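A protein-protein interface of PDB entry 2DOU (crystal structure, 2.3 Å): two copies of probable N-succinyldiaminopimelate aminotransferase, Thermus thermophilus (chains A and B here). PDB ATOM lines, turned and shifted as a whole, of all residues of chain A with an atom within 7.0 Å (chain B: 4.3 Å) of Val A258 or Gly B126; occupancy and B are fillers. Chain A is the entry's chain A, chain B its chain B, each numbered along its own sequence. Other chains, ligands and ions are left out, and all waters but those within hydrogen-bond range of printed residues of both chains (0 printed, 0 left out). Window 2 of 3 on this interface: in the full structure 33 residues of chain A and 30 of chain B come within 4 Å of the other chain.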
ATOM      1  N   LEU A 252     -19.007 -17.749  27.835  1.00  0.00           N
ATOM      2  CA  LEU A 252     -18.804 -18.647  28.958  1.00  0.00           C
ATOM      3  C   LEU A 252     -18.433 -20.040  28.470  1.00  0.00           C
ATOM      4  O   LEU A 252     -17.501 -20.668  28.989  1.00  0.00           O
ATOM      5  CB  LEU A 252     -20.061 -18.726  29.824  1.00  0.00           C
ATOM      6  CG  LEU A 252     -20.038 -19.757  30.961  1.00  0.00           C
ATOM      7  CD1 LEU A 252     -18.825 -19.527  31.860  1.00  0.00           C
ATOM      8  CD2 LEU A 252     -21.336 -19.647  31.762  1.00  0.00           C
ATOM      9  N   GLU A 253     -19.150 -20.510  27.455  1.00  0.00           N
ATOM     10  CA  GLU A 253     -18.906 -21.832  26.899  1.00  0.00           C
ATOM     11  C   GLU A 253     -17.481 -21.951  26.382  1.00  0.00           C
ATOM     12  O   GLU A 253     -16.850 -22.998  26.506  1.00  0.00           O
ATOM     13  CB  GLU A 253     -19.893 -22.129  25.762  1.00  0.00           C
ATOM     14  CG  GLU A 253     -19.799 -23.555  25.235  1.00  0.00           C
ATOM     15  CD  GLU A 253     -20.911 -23.916  24.249  1.00  0.00           C
ATOM     16  OE1 GLU A 253     -21.042 -25.116  23.918  1.00  0.00           O
ATOM     17  OE2 GLU A 253     -21.649 -23.006  23.805  1.00  0.00           O
ATOM     18  N   ARG A 254     -16.984 -20.876  25.791  1.00  0.00           N
ATOM     19  CA  ARG A 254     -15.633 -20.872  25.254  1.00  0.00           C
ATOM     20  C   ARG A 254     -14.592 -20.987  26.383  1.00  0.00           C
ATOM     21  O   ARG A 254     -13.589 -21.680  26.242  1.00  0.00           O
ATOM     22  CB  ARG A 254     -15.428 -19.606  24.410  1.00  0.00           C
ATOM     23  CG  ARG A 254     -13.991 -19.223  24.109  1.00  0.00           C
ATOM     24  CD  ARG A 254     -13.146 -20.380  23.615  1.00  0.00           C
ATOM     25  NE  ARG A 254     -11.743 -19.990  23.502  1.00  0.00           N
ATOM     26  CZ  ARG A 254     -11.086 -19.259  24.409  1.00  0.00           C
ATOM     27  NH1 ARG A 254     -11.687 -18.819  25.515  1.00  0.00           N
ATOM     28  NH2 ARG A 254      -9.811 -18.962  24.206  1.00  0.00           N
ATOM     29  N   VAL A 255     -14.850 -20.330  27.507  1.00  0.00           N
ATOM     30  CA  VAL A 255     -13.940 -20.381  28.653  1.00  0.00           C
ATOM     31  C   VAL A 255     -13.940 -21.768  29.307  1.00  0.00           C
ATOM     32  O   VAL A 255     -12.886 -22.378  29.507  1.00  0.00           O
ATOM     33  CB  VAL A 255     -14.329 -19.326  29.712  1.00  0.00           C
ATOM     34  CG1 VAL A 255     -13.594 -19.596  31.009  1.00  0.00           C
ATOM     35  CG2 VAL A 255     -14.003 -17.935  29.191  1.00  0.00           C
ATOM     36  N   LYS A 256     -15.125 -22.261  29.641  1.00  0.00           N
ATOM     37  CA  LYS A 256     -15.241 -23.573  30.255  1.00  0.00           C
ATOM     38  C   LYS A 256     -14.653 -24.635  29.333  1.00  0.00           C
ATOM     39  O   LYS A 256     -14.142 -25.662  29.797  1.00  0.00           O
ATOM     40  CB  LYS A 256     -16.705 -23.879  30.571  1.00  0.00           C
ATOM     41  CG  LYS A 256     -17.254 -23.064  31.733  1.00  0.00           C
ATOM     42  CD  LYS A 256     -18.740 -23.322  31.985  1.00  0.00           C
ATOM     43  CE  LYS A 256     -19.063 -24.798  32.136  1.00  0.00           C
ATOM     44  NZ  LYS A 256     -18.488 -25.420  33.353  1.00  0.00           N
ATOM     45  N   GLY A 257     -14.712 -24.372  28.027  1.00  0.00           N
ATOM     46  CA  GLY A 257     -14.184 -25.305  27.044  1.00  0.00           C
ATOM     47  C   GLY A 257     -12.680 -25.524  27.124  1.00  0.00           C
ATOM     48  O   GLY A 257     -12.182 -26.584  26.757  1.00  0.00           O
ATOM     49  N   VAL A 258     -11.946 -24.521  27.586  1.00  0.00           N
ATOM     50  CA  VAL A 258     -10.504 -24.658  27.706  1.00  0.00           C
ATOM     51  C   VAL A 258     -10.125 -25.014  29.148  1.00  0.00           C
ATOM     52  O   VAL A 258      -8.963 -25.267  29.440  1.00  0.00           O
ATOM     53  CB  VAL A 258      -9.780 -23.354  27.283  1.00  0.00           C
ATOM     54  CG1 VAL A 258     -10.057 -23.058  25.822  1.00  0.00           C
ATOM     55  CG2 VAL A 258     -10.226 -22.199  28.147  1.00  0.00           C
ATOM     56  N   ILE A 259     -11.119 -25.059  30.030  1.00  0.00           N
ATOM     57  CA  ILE A 259     -10.907 -25.357  31.442  1.00  0.00           C
ATOM     58  C   ILE A 259     -11.460 -26.701  31.931  1.00  0.00           C
ATOM     59  O   ILE A 259     -10.834 -27.363  32.760  1.00  0.00           O
ATOM     60  CB  ILE A 259     -11.498 -24.227  32.322  1.00  0.00           C
ATOM     61  CG1 ILE A 259     -10.693 -22.944  32.109  1.00  0.00           C
ATOM     62  CG2 ILE A 259     -11.514 -24.629  33.783  1.00  0.00           C
ATOM     63  CD1 ILE A 259     -11.199 -21.756  32.905  1.00  0.00           C
ATOM     64  N   ASP A 260     -12.617 -27.115  31.420  1.00  0.00           N
ATOM     65  CA  ASP A 260     -13.211 -28.372  31.861  1.00  0.00           C
ATOM     66  C   ASP A 260     -13.905 -29.184  30.763  1.00  0.00           C
ATOM     67  O   ASP A 260     -13.798 -28.885  29.571  1.00  0.00           O
ATOM     68  CB  ASP A 260     -14.208 -28.099  32.992  1.00  0.00           C
ATOM     69  CG  ASP A 260     -15.478 -27.402  32.502  1.00  0.00           C
ATOM     70  OD1 ASP A 260     -16.271 -28.045  31.771  1.00  0.00           O
ATOM     71  OD2 ASP A 260     -15.678 -26.213  32.841  1.00  0.00           O
ATOM     72  N   GLN B  97      -7.214 -30.716  33.412  1.00  0.00           N
ATOM     73  CA  GLN B  97      -7.361 -29.531  32.556  1.00  0.00           C
ATOM     74  C   GLN B  97      -7.740 -28.311  33.399  1.00  0.00           C
ATOM     75  O   GLN B  97      -7.306 -27.187  33.143  1.00  0.00           O
ATOM     76  CB  GLN B  97      -8.423 -29.768  31.470  1.00  0.00           C
ATOM     77  CG  GLN B  97      -8.507 -28.629  30.467  1.00  0.00           C
ATOM     78  CD  GLN B  97      -9.264 -28.998  29.190  1.00  0.00           C
ATOM     79  OE1 GLN B  97     -10.479 -29.220  29.207  1.00  0.00           O
ATOM     80  NE2 GLN B  97      -8.537 -29.064  28.077  1.00  0.00           N
ATOM     81  N   PRO B 122      -4.321 -28.242  22.473  1.00  0.00           N
ATOM     82  CA  PRO B 122      -5.089 -27.037  22.125  1.00  0.00           C
ATOM     83  C   PRO B 122      -5.495 -26.115  23.275  1.00  0.00           C
ATOM     84  O   PRO B 122      -5.280 -24.903  23.206  1.00  0.00           O
ATOM     85  CB  PRO B 122      -6.294 -27.604  21.377  1.00  0.00           C
ATOM     86  CG  PRO B 122      -5.705 -28.810  20.697  1.00  0.00           C
ATOM     87  CD  PRO B 122      -4.884 -29.427  21.802  1.00  0.00           C
ATOM     88  N   SER B 123      -6.071 -26.671  24.332  1.00  0.00           N
ATOM     89  CA  SER B 123      -6.488 -25.829  25.441  1.00  0.00           C
ATOM     90  C   SER B 123      -5.362 -25.113  26.196  1.00  0.00           C
ATOM     91  O   SER B 123      -5.637 -24.210  26.984  1.00  0.00           O
ATOM     92  CB  SER B 123      -7.356 -26.621  26.412  1.00  0.00           C
ATOM     93  OG  SER B 123      -6.755 -27.845  26.744  1.00  0.00           O
ATOM     94  N   TYR B 124      -4.106 -25.490  25.962  1.00  0.00           N
ATOM     95  CA  TYR B 124      -3.008 -24.796  26.634  1.00  0.00           C
ATOM     96  C   TYR B 124      -3.043 -23.351  26.170  1.00  0.00           C
ATOM     97  O   TYR B 124      -3.049 -22.430  26.980  1.00  0.00           O
ATOM     98  CB  TYR B 124      -1.642 -25.393  26.278  1.00  0.00           C
ATOM     99  CG  TYR B 124      -1.322 -26.723  26.921  1.00  0.00           C
ATOM    100  CD1 TYR B 124      -0.089 -27.340  26.699  1.00  0.00           C
ATOM    101  CD2 TYR B 124      -2.245 -27.374  27.734  1.00  0.00           C
ATOM    102  CE1 TYR B 124       0.215 -28.578  27.269  1.00  0.00           C
ATOM    103  CE2 TYR B 124      -1.952 -28.613  28.306  1.00  0.00           C
ATOM    104  CZ  TYR B 124      -0.721 -29.209  28.064  1.00  0.00           C
ATOM    105  OH  TYR B 124      -0.453 -30.454  28.571  1.00  0.00           O
ATOM    106  N   PHE B 125      -3.067 -23.154  24.856  1.00  0.00           N
ATOM    107  CA  PHE B 125      -3.111 -21.808  24.300  1.00  0.00           C
ATOM    108  C   PHE B 125      -4.350 -21.087  24.840  1.00  0.00           C
ATOM    109  O   PHE B 125      -4.306 -19.897  25.140  1.00  0.00           O
ATOM    110  CB  PHE B 125      -3.146 -21.859  22.765  1.00  0.00           C
ATOM    111  CG  PHE B 125      -2.083 -22.737  22.156  1.00  0.00           C
ATOM    112  CD1 PHE B 125      -2.375 -24.043  21.776  1.00  0.00           C
ATOM    113  CD2 PHE B 125      -0.787 -22.264  21.979  1.00  0.00           C
ATOM    114  CE1 PHE B 125      -1.394 -24.867  21.225  1.00  0.00           C
ATOM    115  CE2 PHE B 125       0.205 -23.080  21.430  1.00  0.00           C
ATOM    116  CZ  PHE B 125      -0.099 -24.384  21.052  1.00  0.00           C
ATOM    117  N   GLY B 126      -5.454 -21.820  24.970  1.00  0.00           N
ATOM    118  CA  GLY B 126      -6.674 -21.231  25.486  1.00  0.00           C
ATOM    119  C   GLY B 126      -6.502 -20.776  26.922  1.00  0.00           C
ATOM    120  O   GLY B 126      -6.790 -19.628  27.253  1.00  0.00           O
ATOM    121  N   ALA B 127      -6.035 -21.679  27.779  1.00  0.00           N
ATOM    122  CA  ALA B 127      -5.817 -21.355  29.190  1.00  0.00           C
ATOM    123  C   ALA B 127      -4.937 -20.116  29.281  1.00  0.00           C
ATOM    124  O   ALA B 127      -5.123 -19.271  30.151  1.00  0.00           O
ATOM    125  CB  ALA B 127      -5.158 -22.526  29.903  1.00  0.00           C
ATOM    126  N   ALA B 128      -3.988 -20.017  28.360  1.00  0.00           N
ATOM    127  CA  ALA B 128      -3.082 -18.879  28.302  1.00  0.00           C
ATOM    128  C   ALA B 128      -3.865 -17.590  28.036  1.00  0.00           C
ATOM    129  O   ALA B 128      -3.636 -16.570  28.693  1.00  0.00           O
ATOM    130  CB  ALA B 128      -2.050 -19.096  27.215  1.00  0.00           C
ATOM    131  N   ARG B 129      -4.792 -17.630  27.076  1.00  0.00           N
ATOM    132  CA  ARG B 129      -5.592 -16.443  26.770  1.00  0.00           C
ATOM    133  C   ARG B 129      -6.523 -16.111  27.936  1.00  0.00           C
ATOM    134  O   ARG B 129      -6.750 -14.948  28.235  1.00  0.00           O
ATOM    135  CB  ARG B 129      -6.399 -16.654  25.484  1.00  0.00           C
ATOM    136  N   VAL B 130      -7.044 -17.134  28.605  1.00  0.00           N
ATOM    137  CA  VAL B 130      -7.941 -16.918  29.739  1.00  0.00           C
ATOM    138  C   VAL B 130      -7.247 -16.154  30.865  1.00  0.00           C
ATOM    139  O   VAL B 130      -7.872 -15.359  31.570  1.00  0.00           O
ATOM    140  CB  VAL B 130      -8.451 -18.257  30.314  1.00  0.00           C
ATOM    141  CG1 VAL B 130      -9.310 -18.015  31.542  1.00  0.00           C
ATOM    142  CG2 VAL B 130      -9.240 -18.998  29.262  1.00  0.00           C
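Glu A253 touches none of the printed residues of chain B. Printed residues of chain B within 4 Å of Gly A257: Gln B97. Val A258 touches just these residues of chain B: Gln B97 (3.5 Å), Ser B123 (3.7 Å), Gly B126 (3.9 Å) and Val B130 (3.5 Å). Of the printed residues of chain B, Ile A259 touches Gln B97 (3.3 Å). Of chain A, only Val A258 comes within 4 Å of Gly B126. The nearest residue of chain A that does not touch Gly B126 is Arg A254 (4.1 Å). The nearest printed residue of chain B that does not touch Gly A257 is Ser B123 (4.8 Å).
Gln B97 touches Gly A257 (OE1 to O, 3.98 Å). Gln B97 touches Val A258 (CG to O, 3.5 Å). Ser B123 touches Val A258 (CB to O, 3.7 Å). CA of Gly B126 touches CG1 of Val A258, at 3.9 Å. Val B130 touches Val A258. Gln B97 touches Ile A259 (C to O, 3.3 Å).
The side-chain amide oxygen of Gln B97 lies close to the backbone carbonyl oxygen of Asp A260 (3.4 Å).
The side-chain carboxylate of Asp A260 lies within salt-bridge range of the side-chain amino group of Lys A256, at 3.0 Å. The side-chain amide nitrogen (NE2) of Gln B97 is in hydrogen-bond range of the side-chain hydroxyl (OG) of Ser B123 (2.5 Å).
No position is printed for both chains.
Of the 9 printed residues of chain A, 4 touch a printed residue of chain B. Hydrophobic or aromatic side chains of chain A that line the printed part of chain B: Val A258. Printed residues of chain B that touch a printed residue of chain A: Gln B97, Ser B123, Gly B126 and Val B130. Hydrophobic or aromatic side chains of chain B that line the printed part of chain A: Val B130. Among the printed residues, no Asp or Glu carboxylate lies within 4 Å of a Lys or Arg side-chain nitrogen of the other chain.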
